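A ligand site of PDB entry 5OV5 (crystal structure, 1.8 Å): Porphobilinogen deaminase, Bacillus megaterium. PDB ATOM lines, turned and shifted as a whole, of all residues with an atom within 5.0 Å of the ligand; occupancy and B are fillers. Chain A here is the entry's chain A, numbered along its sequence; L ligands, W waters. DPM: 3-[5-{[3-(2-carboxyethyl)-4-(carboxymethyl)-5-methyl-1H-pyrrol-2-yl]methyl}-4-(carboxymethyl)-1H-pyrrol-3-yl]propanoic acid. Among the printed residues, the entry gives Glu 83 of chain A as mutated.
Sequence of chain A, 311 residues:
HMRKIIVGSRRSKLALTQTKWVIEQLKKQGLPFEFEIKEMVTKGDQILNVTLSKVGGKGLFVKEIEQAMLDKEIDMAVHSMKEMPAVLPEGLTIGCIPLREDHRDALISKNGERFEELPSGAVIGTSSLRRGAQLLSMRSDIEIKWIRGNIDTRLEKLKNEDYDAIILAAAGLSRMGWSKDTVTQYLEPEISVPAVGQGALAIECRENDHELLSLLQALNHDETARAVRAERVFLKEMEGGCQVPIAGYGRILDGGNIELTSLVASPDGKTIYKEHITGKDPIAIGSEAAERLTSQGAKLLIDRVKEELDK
A carbon (CHA) of the ligand is covalently linked to the side-chain sulfur (SG) of Cys 242 (1.8 Å).
The side-chain hydroxyl (OG) of Ser 80 lies within hydrogen-bond range of an oxygen (O3B) of the ligand (2.4 Å).
The side-chain amino group (NZ) of Lys 82 lies within salt-bridge range of an oxygen (O2B) of the ligand, 2.5 Å away.
O2A of the ligand is in salt-bridge range of NE of Arg 130 (2.6 Å).
An oxygen (O3A) of the ligand is in hydrogen-bond range of the backbone NH of Ser 127.
OG of Ser 127 is in hydrogen-bond range of O3A of the ligand (2.7 Å).
NH1 of Arg 154 lies within salt-bridge range of O3A of the ligand (2.7 Å).
A nitrogen (NB) of the ligand is in hydrogen-bond range of the side-chain carboxylate (OE2) of Glu 83 (2.8 Å).
The side-chain hydroxyl of Thr 126 is in hydrogen-bond range of an oxygen (O4A) of the ligand, at 2.8 Å.
NH1 of Arg 131 is in salt-bridge range of O4A of the ligand (2.8 Å).
An oxygen (O1B) of the ligand sits at hydrogen-bond distance from the backbone NH (N) of Ala 169, 3.0 Å away.
The side-chain hydroxyl (OG) of Ser 128 lies within hydrogen-bond range of an oxygen (O2A) of the ligand, at 3.2 Å.
O4B of the ligand sits at hydrogen-bond distance from N of Gly 199, 3.3 Å away.
The side-chain hydroxyl of Ser 80 is in hydrogen-bond range of the side-chain amide nitrogen of Gln 18, 3.2 Å away.
NZ of Lys 82 sits at hydrogen-bond distance from OE1 of Gln 198 (2.9 Å).
OG of Ser 128 sits close to N of Arg 130, 3.3 Å away.
OG1 of Thr 126 lies within hydrogen-bond range of N of Ser 128 (3.0 Å).
The backbone NH (N) of Arg 131 lies within hydrogen-bond range of the side-chain hydroxyl (OG) of Ser 128 (3.0 Å).
The guanidinium group (NH2) of Arg 131 is in hydrogen-bond range of the side-chain amide oxygen (OE1) of Gln 198 (3.0 Å).
O of Gly 199 sits at hydrogen-bond distance from NH2 of Arg 175 (2.9 Å).
The side-chain amide nitrogen (NE2) of Gln 18 sits close to the guanidinium group (NH1) of Arg 175 (3.5 Å).
Residues that only touch the ligand: Leu 14, Gln 18, Leu 168, Ala 195 and Gln 198.
Hydrophobic or aromatic side chains that line the ligand: Leu 14, Leu 168, Ala 169 and Ala 195.
The nearest printed residue that does not touch the ligand is Gly 172 (4.01 Å).
Water W1 lies within hydrogen-bond range of the backbone NH of Lys 82 (2.9 Å), an oxygen (O4B) of the ligand (2.9 Å) and the backbone carbonyl oxygen of Gly 197 (3.0 Å).
Water W2 lies within hydrogen-bond range of the backbone carbonyl oxygen of Cys 242, the backbone NH of Arg 130, the side-chain hydroxyl of Ser 128 and an oxygen (O2A) of the ligand.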
ATOM      1  N   LEU A  14     -12.583   7.189  29.958  1.00  0.00           N
ATOM      2  CA  LEU A  14     -12.670   8.559  29.466  1.00  0.00           C
ATOM      3  C   LEU A  14     -13.475   9.426  30.414  1.00  0.00           C
ATOM      4  O   LEU A  14     -13.071  10.552  30.726  1.00  0.00           O
ATOM      5  CB  LEU A  14     -13.257   8.582  28.062  1.00  0.00           C
ATOM      6  CG  LEU A  14     -13.356   9.953  27.384  1.00  0.00           C
ATOM      7  CD1 LEU A  14     -12.005  10.648  27.311  1.00  0.00           C
ATOM      8  CD2 LEU A  14     -13.974   9.827  25.989  1.00  0.00           C
ATOM      9  N   GLN A  18     -11.948  12.652  32.443  1.00  0.00           N
ATOM     10  CA  GLN A  18     -12.529  13.993  32.365  1.00  0.00           C
ATOM     11  C   GLN A  18     -12.966  14.492  33.736  1.00  0.00           C
ATOM     12  O   GLN A  18     -12.766  15.669  34.064  1.00  0.00           O
ATOM     13  CB  GLN A  18     -13.734  13.998  31.409  1.00  0.00           C
ATOM     14  CG  GLN A  18     -13.355  13.795  29.972  1.00  0.00           C
ATOM     15  CD  GLN A  18     -14.558  13.587  29.074  1.00  0.00           C
ATOM     16  OE1 GLN A  18     -15.673  13.382  29.545  1.00  0.00           O
ATOM     17  NE2 GLN A  18     -14.328  13.633  27.778  1.00  0.00           N
ATOM     18  N   SER A  80     -19.168  14.803  28.570  1.00  0.00           N
ATOM     19  CA  SER A  80     -18.894  15.306  27.219  1.00  0.00           C
ATOM     20  C   SER A  80     -20.106  16.080  26.737  1.00  0.00           C
ATOM     21  O   SER A  80     -21.230  15.563  26.781  1.00  0.00           O
ATOM     22  CB  SER A  80     -18.592  14.149  26.253  1.00  0.00           C
ATOM     23  OG  SER A  80     -17.292  13.634  26.472  1.00  0.00           O
ATOM     24  N   LYS A  82     -21.216  16.702  23.866  1.00  0.00           N
ATOM     25  CA  LYS A  82     -22.029  16.105  22.814  1.00  0.00           C
ATOM     26  C   LYS A  82     -22.889  14.954  23.318  1.00  0.00           C
ATOM     27  O   LYS A  82     -23.772  14.502  22.576  1.00  0.00           O
ATOM     28  CB  LYS A  82     -21.161  15.651  21.628  1.00  0.00           C
ATOM     29  CG  LYS A  82     -20.223  14.489  21.881  1.00  0.00           C
ATOM     30  CD  LYS A  82     -19.806  13.933  20.510  1.00  0.00           C
ATOM     31  CE  LYS A  82     -18.865  12.760  20.623  1.00  0.00           C
ATOM     32  NZ  LYS A  82     -18.511  12.300  19.235  1.00  0.00           N
ATOM     33  N   GLU A  83     -22.683  14.510  24.562  1.00  0.00           N
ATOM     34  CA  GLU A  83     -23.537  13.516  25.208  1.00  0.00           C
ATOM     35  C   GLU A  83     -24.641  14.133  26.046  1.00  0.00           C
ATOM     36  O   GLU A  83     -25.495  13.389  26.547  1.00  0.00           O
ATOM     37  CB  GLU A  83     -22.710  12.601  26.130  1.00  0.00           C
ATOM     38  CG  GLU A  83     -21.637  11.780  25.435  1.00  0.00           C
ATOM     39  CD  GLU A  83     -22.188  10.516  24.803  1.00  0.00           C
ATOM     40  OE1 GLU A  83     -23.284  10.058  25.223  1.00  0.00           O
ATOM     41  OE2 GLU A  83     -21.522   9.956  23.898  1.00  0.00           O
ATOM     42  N   THR A 126     -17.578   3.588  11.944  1.00  0.00           N
ATOM     43  CA  THR A 126     -18.193   4.547  12.857  1.00  0.00           C
ATOM     44  C   THR A 126     -19.671   4.196  12.983  1.00  0.00           C
ATOM     45  O   THR A 126     -20.319   3.863  11.994  1.00  0.00           O
ATOM     46  CB  THR A 126     -18.029   6.000  12.368  1.00  0.00           C
ATOM     47  OG1 THR A 126     -18.901   6.847  13.118  1.00  0.00           O
ATOM     48  CG2 THR A 126     -18.407   6.140  10.920  1.00  0.00           C
ATOM     49  N   SER A 127     -20.195   4.252  14.209  1.00  0.00           N
ATOM     50  CA  SER A 127     -21.629   4.041  14.388  1.00  0.00           C
ATOM     51  C   SER A 127     -22.423   5.333  14.272  1.00  0.00           C
ATOM     52  O   SER A 127     -23.654   5.302  14.420  1.00  0.00           O
ATOM     53  CB  SER A 127     -21.927   3.395  15.741  1.00  0.00           C
ATOM     54  OG  SER A 127     -21.717   4.328  16.804  1.00  0.00           O
ATOM     55  N   SER A 128     -21.750   6.461  14.006  1.00  0.00           N
ATOM     56  CA  SER A 128     -22.385   7.769  13.949  1.00  0.00           C
ATOM     57  C   SER A 128     -22.925   8.036  12.550  1.00  0.00           C
ATOM     58  O   SER A 128     -22.155   8.117  11.588  1.00  0.00           O
ATOM     59  CB  SER A 128     -21.386   8.858  14.344  1.00  0.00           C
ATOM     60  OG  SER A 128     -21.869  10.144  13.972  1.00  0.00           O
ATOM     61  N   ARG A 130     -24.188  10.909  11.741  1.00  0.00           N
ATOM     62  CA  ARG A 130     -23.640  12.228  11.440  1.00  0.00           C
ATOM     63  C   ARG A 130     -22.312  12.126  10.701  1.00  0.00           C
ATOM     64  O   ARG A 130     -22.092  12.822   9.680  1.00  0.00           O
ATOM     65  CB  ARG A 130     -23.456  13.016  12.739  1.00  0.00           C
ATOM     66  CG  ARG A 130     -22.700  14.299  12.509  1.00  0.00           C
ATOM     67  CD  ARG A 130     -22.329  14.962  13.838  1.00  0.00           C
ATOM     68  NE  ARG A 130     -21.236  14.318  14.582  1.00  0.00           N
ATOM     69  CZ  ARG A 130     -19.930  14.348  14.268  1.00  0.00           C
ATOM     70  NH1 ARG A 130     -19.510  14.899  13.110  1.00  0.00           N
ATOM     71  NH2 ARG A 130     -19.035  13.791  15.091  1.00  0.00           N
ATOM     72  N   ARG A 131     -21.391  11.323  11.234  1.00  0.00           N
ATOM     73  CA  ARG A 131     -20.086  11.145  10.595  1.00  0.00           C
ATOM     74  C   ARG A 131     -20.234  10.412   9.262  1.00  0.00           C
ATOM     75  O   ARG A 131     -19.727  10.869   8.232  1.00  0.00           O
ATOM     76  CB  ARG A 131     -19.146  10.371  11.535  1.00  0.00           C
ATOM     77  CG  ARG A 131     -18.643  11.238  12.666  1.00  0.00           C
ATOM     78  CD  ARG A 131     -17.948  10.427  13.729  1.00  0.00           C
ATOM     79  NE  ARG A 131     -17.238  11.324  14.627  1.00  0.00           N
ATOM     80  CZ  ARG A 131     -16.749  10.957  15.807  1.00  0.00           C
ATOM     81  NH1 ARG A 131     -16.908   9.718  16.244  1.00  0.00           N
ATOM     82  NH2 ARG A 131     -16.108  11.847  16.557  1.00  0.00           N
ATOM     83  N   ILE A 147     -19.233   0.136  14.368  1.00  0.00           N
ATOM     84  CA  ILE A 147     -18.122  -0.366  15.162  1.00  0.00           C
ATOM     85  C   ILE A 147     -18.390   0.095  16.588  1.00  0.00           C
ATOM     86  O   ILE A 147     -19.012   1.130  16.802  1.00  0.00           O
ATOM     87  CB  ILE A 147     -16.749   0.130  14.627  1.00  0.00           C
ATOM     88  CG1 ILE A 147     -15.585  -0.566  15.325  1.00  0.00           C
ATOM     89  CG2 ILE A 147     -16.616   1.647  14.770  1.00  0.00           C
ATOM     90  CD1 ILE A 147     -14.201  -0.070  14.886  1.00  0.00           C
ATOM     91  N   ARG A 154     -11.311   0.346  19.533  1.00  0.00           N
ATOM     92  CA  ARG A 154     -11.483   0.612  18.103  1.00  0.00           C
ATOM     93  C   ARG A 154     -10.148   0.659  17.381  1.00  0.00           C
ATOM     94  O   ARG A 154     -10.038   0.197  16.234  1.00  0.00           O
ATOM     95  CB  ARG A 154     -12.267   1.911  17.897  1.00  0.00           C
ATOM     96  CG  ARG A 154     -13.646   1.904  18.556  1.00  0.00           C
ATOM     97  CD  ARG A 154     -14.495   3.099  18.101  1.00  0.00           C
ATOM     98  NE  ARG A 154     -15.811   3.136  18.726  1.00  0.00           N
ATOM     99  CZ  ARG A 154     -16.860   3.800  18.238  1.00  0.00           C
ATOM    100  NH1 ARG A 154     -16.756   4.486  17.107  1.00  0.00           N
ATOM    101  NH2 ARG A 154     -18.018   3.772  18.888  1.00  0.00           N
ATOM    102  N   ILE A 167     -13.227   6.636  12.420  1.00  0.00           N
ATOM    103  CA  ILE A 167     -13.342   8.042  12.776  1.00  0.00           C
ATOM    104  C   ILE A 167     -13.444   8.118  14.294  1.00  0.00           C
ATOM    105  O   ILE A 167     -14.250   7.410  14.904  1.00  0.00           O
ATOM    106  CB  ILE A 167     -14.567   8.739  12.150  1.00  0.00           C
ATOM    107  CG1 ILE A 167     -14.645   8.531  10.630  1.00  0.00           C
ATOM    108  CG2 ILE A 167     -14.604  10.245  12.525  1.00  0.00           C
ATOM    109  CD1 ILE A 167     -13.513   9.171   9.817  1.00  0.00           C
ATOM    110  N   LEU A 168     -12.668   9.027  14.897  1.00  0.00           N
ATOM    111  CA  LEU A 168     -12.747   9.279  16.332  1.00  0.00           C
ATOM    112  C   LEU A 168     -12.700  10.783  16.577  1.00  0.00           C
ATOM    113  O   LEU A 168     -12.208  11.543  15.740  1.00  0.00           O
ATOM    114  CB  LEU A 168     -11.596   8.611  17.087  1.00  0.00           C
ATOM    115  CG  LEU A 168     -11.408   7.099  16.955  1.00  0.00           C
ATOM    116  CD1 LEU A 168     -10.051   6.709  17.506  1.00  0.00           C
ATOM    117  CD2 LEU A 168     -12.508   6.339  17.669  1.00  0.00           C
ATOM    118  N   ALA A 169     -13.168  11.208  17.748  1.00  0.00           N
ATOM    119  CA  ALA A 169     -13.003  12.619  18.100  1.00  0.00           C
ATOM    120  C   ALA A 169     -11.545  12.890  18.457  1.00  0.00           C
ATOM    121  O   ALA A 169     -10.942  12.173  19.274  1.00  0.00           O
ATOM    122  CB  ALA A 169     -13.917  12.991  19.260  1.00  0.00           C
ATOM    123  N   ALA A 171     -10.617  15.170  20.315  1.00  0.00           N
ATOM    124  CA  ALA A 171     -10.647  15.513  21.727  1.00  0.00           C
ATOM    125  C   ALA A 171     -10.489  14.291  22.625  1.00  0.00           C
ATOM    126  O   ALA A 171      -9.780  14.339  23.629  1.00  0.00           O
ATOM    127  CB  ALA A 171     -11.956  16.236  22.077  1.00  0.00           C
ATOM    128  N   GLY A 172     -11.165  13.188  22.288  1.00  0.00           N
ATOM    129  CA  GLY A 172     -11.027  11.970  23.070  1.00  0.00           C
ATOM    130  C   GLY A 172      -9.641  11.357  22.938  1.00  0.00           C
ATOM    131  O   GLY A 172      -9.089  10.867  23.922  1.00  0.00           O
ATOM    132  N   ARG A 175      -7.450  13.616  25.207  1.00  0.00           N
ATOM    133  CA  ARG A 175      -7.690  13.404  26.632  1.00  0.00           C
ATOM    134  C   ARG A 175      -7.215  12.026  27.103  1.00  0.00           C
ATOM    135  O   ARG A 175      -6.815  11.874  28.264  1.00  0.00           O
ATOM    136  CB  ARG A 175      -9.175  13.613  26.967  1.00  0.00           C
ATOM    137  CG  ARG A 175      -9.634  15.071  26.806  1.00  0.00           C
ATOM    138  CD  ARG A 175     -11.003  15.367  27.458  1.00  0.00           C
ATOM    139  NE  ARG A 175     -11.400  16.775  27.262  1.00  0.00           N
ATOM    140  CZ  ARG A 175     -12.431  17.178  26.511  1.00  0.00           C
ATOM    141  NH1 ARG A 175     -13.195  16.293  25.892  1.00  0.00           N
ATOM    142  NH2 ARG A 175     -12.710  18.479  26.394  1.00  0.00           N
ATOM    143  N   ALA A 195     -20.072  17.031  15.700  1.00  0.00           N
ATOM    144  CA  ALA A 195     -21.224  16.987  16.593  1.00  0.00           C
ATOM    145  C   ALA A 195     -21.281  18.250  17.443  1.00  0.00           C
ATOM    146  O   ALA A 195     -20.250  18.789  17.861  1.00  0.00           O
ATOM    147  CB  ALA A 195     -21.157  15.776  17.504  1.00  0.00           C
ATOM    148  N   GLY A 197     -21.176  20.486  20.397  1.00  0.00           N
ATOM    149  CA  GLY A 197     -20.420  20.348  21.619  1.00  0.00           C
ATOM    150  C   GLY A 197     -19.184  19.467  21.592  1.00  0.00           C
ATOM    151  O   GLY A 197     -18.557  19.296  22.630  1.00  0.00           O
ATOM    152  N   GLN A 198     -18.800  18.908  20.446  1.00  0.00           N
ATOM    153  CA  GLN A 198     -17.638  18.036  20.428  1.00  0.00           C
ATOM    154  C   GLN A 198     -16.398  18.791  20.880  1.00  0.00           C
ATOM    155  O   GLN A 198     -16.176  19.934  20.460  1.00  0.00           O
ATOM    156  CB  GLN A 198     -17.441  17.461  19.023  1.00  0.00           C
ATOM    157  CG  GLN A 198     -16.315  16.399  18.965  1.00  0.00           C
ATOM    158  CD  GLN A 198     -16.464  15.480  17.767  1.00  0.00           C
ATOM    159  OE1 GLN A 198     -17.085  14.415  17.855  1.00  0.00           O
ATOM    160  NE2 GLN A 198     -15.879  15.886  16.637  1.00  0.00           N
ATOM    161  N   GLY A 199     -15.601  18.180  21.748  1.00  0.00           N
ATOM    162  CA  GLY A 199     -14.446  18.841  22.328  1.00  0.00           C
ATOM    163  C   GLY A 199     -14.746  19.684  23.568  1.00  0.00           C
ATOM    164  O   GLY A 199     -13.802  20.091  24.262  1.00  0.00           O
ATOM    165  N   CYS A 242     -27.634  12.534  19.781  1.00  0.00           N
ATOM    166  CA  CYS A 242     -26.547  11.633  19.375  1.00  0.00           C
ATOM    167  C   CYS A 242     -26.906  10.804  18.147  1.00  0.00           C
ATOM    168  O   CYS A 242     -26.090  10.665  17.225  1.00  0.00           O
ATOM    169  CB  CYS A 242     -26.220  10.692  20.531  1.00  0.00           C
ATOM    170  SG  CYS A 242     -24.742  11.107  21.386  1.00  0.00           S
HETATM  171  C1A DPM L   1     -22.100  10.573  20.142  1.00  0.00           C
HETATM  172  C2A DPM L   1     -21.600  10.243  18.951  1.00  0.00           C
HETATM  173  C3A DPM L   1     -20.521   9.455  19.173  1.00  0.00           C
HETATM  174  C4A DPM L   1     -20.364   9.360  20.518  1.00  0.00           C
HETATM  175  C5A DPM L   1     -22.240  10.637  17.589  1.00  0.00           C
HETATM  176  C6A DPM L   1     -21.617  11.859  16.842  1.00  0.00           C
HETATM  177  C7A DPM L   1     -19.619   8.820  18.065  1.00  0.00           C
HETATM  178  C8A DPM L   1     -20.021   7.378  17.746  1.00  0.00           C
HETATM  179  C9A DPM L   1     -19.187   6.720  16.613  1.00  0.00           C
HETATM  180  CHA DPM L   1     -23.335  11.447  20.385  1.00  0.00           C
HETATM  181  NA  DPM L   1     -21.344  10.050  21.123  1.00  0.00           N
HETATM  182  O1A DPM L   1     -20.410  12.104  17.033  1.00  0.00           O
HETATM  183  O2A DPM L   1     -22.389  12.490  16.066  1.00  0.00           O
HETATM  184  O3A DPM L   1     -19.250   5.468  16.537  1.00  0.00           O
HETATM  185  O4A DPM L   1     -18.544   7.446  15.804  1.00  0.00           O
HETATM  186  C1B DPM L   1     -18.441   9.625  22.127  1.00  0.00           C
HETATM  187  C2B DPM L   1     -17.128   9.860  22.008  1.00  0.00           C
HETATM  188  C3B DPM L   1     -16.814  10.814  22.885  1.00  0.00           C
HETATM  189  C4B DPM L   1     -17.916  11.191  23.536  1.00  0.00           C
HETATM  190  C5B DPM L   1     -16.152   9.115  21.076  1.00  0.00           C
HETATM  191  C6B DPM L   1     -15.844   9.740  19.699  1.00  0.00           C
HETATM  192  C7B DPM L   1     -15.396  11.402  23.089  1.00  0.00           C
HETATM  193  C8B DPM L   1     -15.147  12.822  22.521  1.00  0.00           C
HETATM  194  CHB DPM L   1     -19.263   8.604  21.314  1.00  0.00           C
HETATM  195  NB  DPM L   1     -18.935  10.447  23.055  1.00  0.00           N
HETATM  196  O1B DPM L   1     -14.924   9.219  19.048  1.00  0.00           O
HETATM  197  O2B DPM L   1     -16.529  10.712  19.314  1.00  0.00           O
HETATM  198  O3B DPM L   1     -16.178  13.936  24.348  1.00  0.00           O
HETATM  199  O4B DPM L   1     -16.167  15.018  22.420  1.00  0.00           O
HETATM  200  O   HOH W   1     -18.354  16.513  23.693  1.00  0.00           O
HETATM  201  O   HOH W   2     -24.921  10.715  14.578  1.00  0.00           O
HETATM  202  O   HOH W   3     -15.289   7.247  23.900  1.00  0.00           O
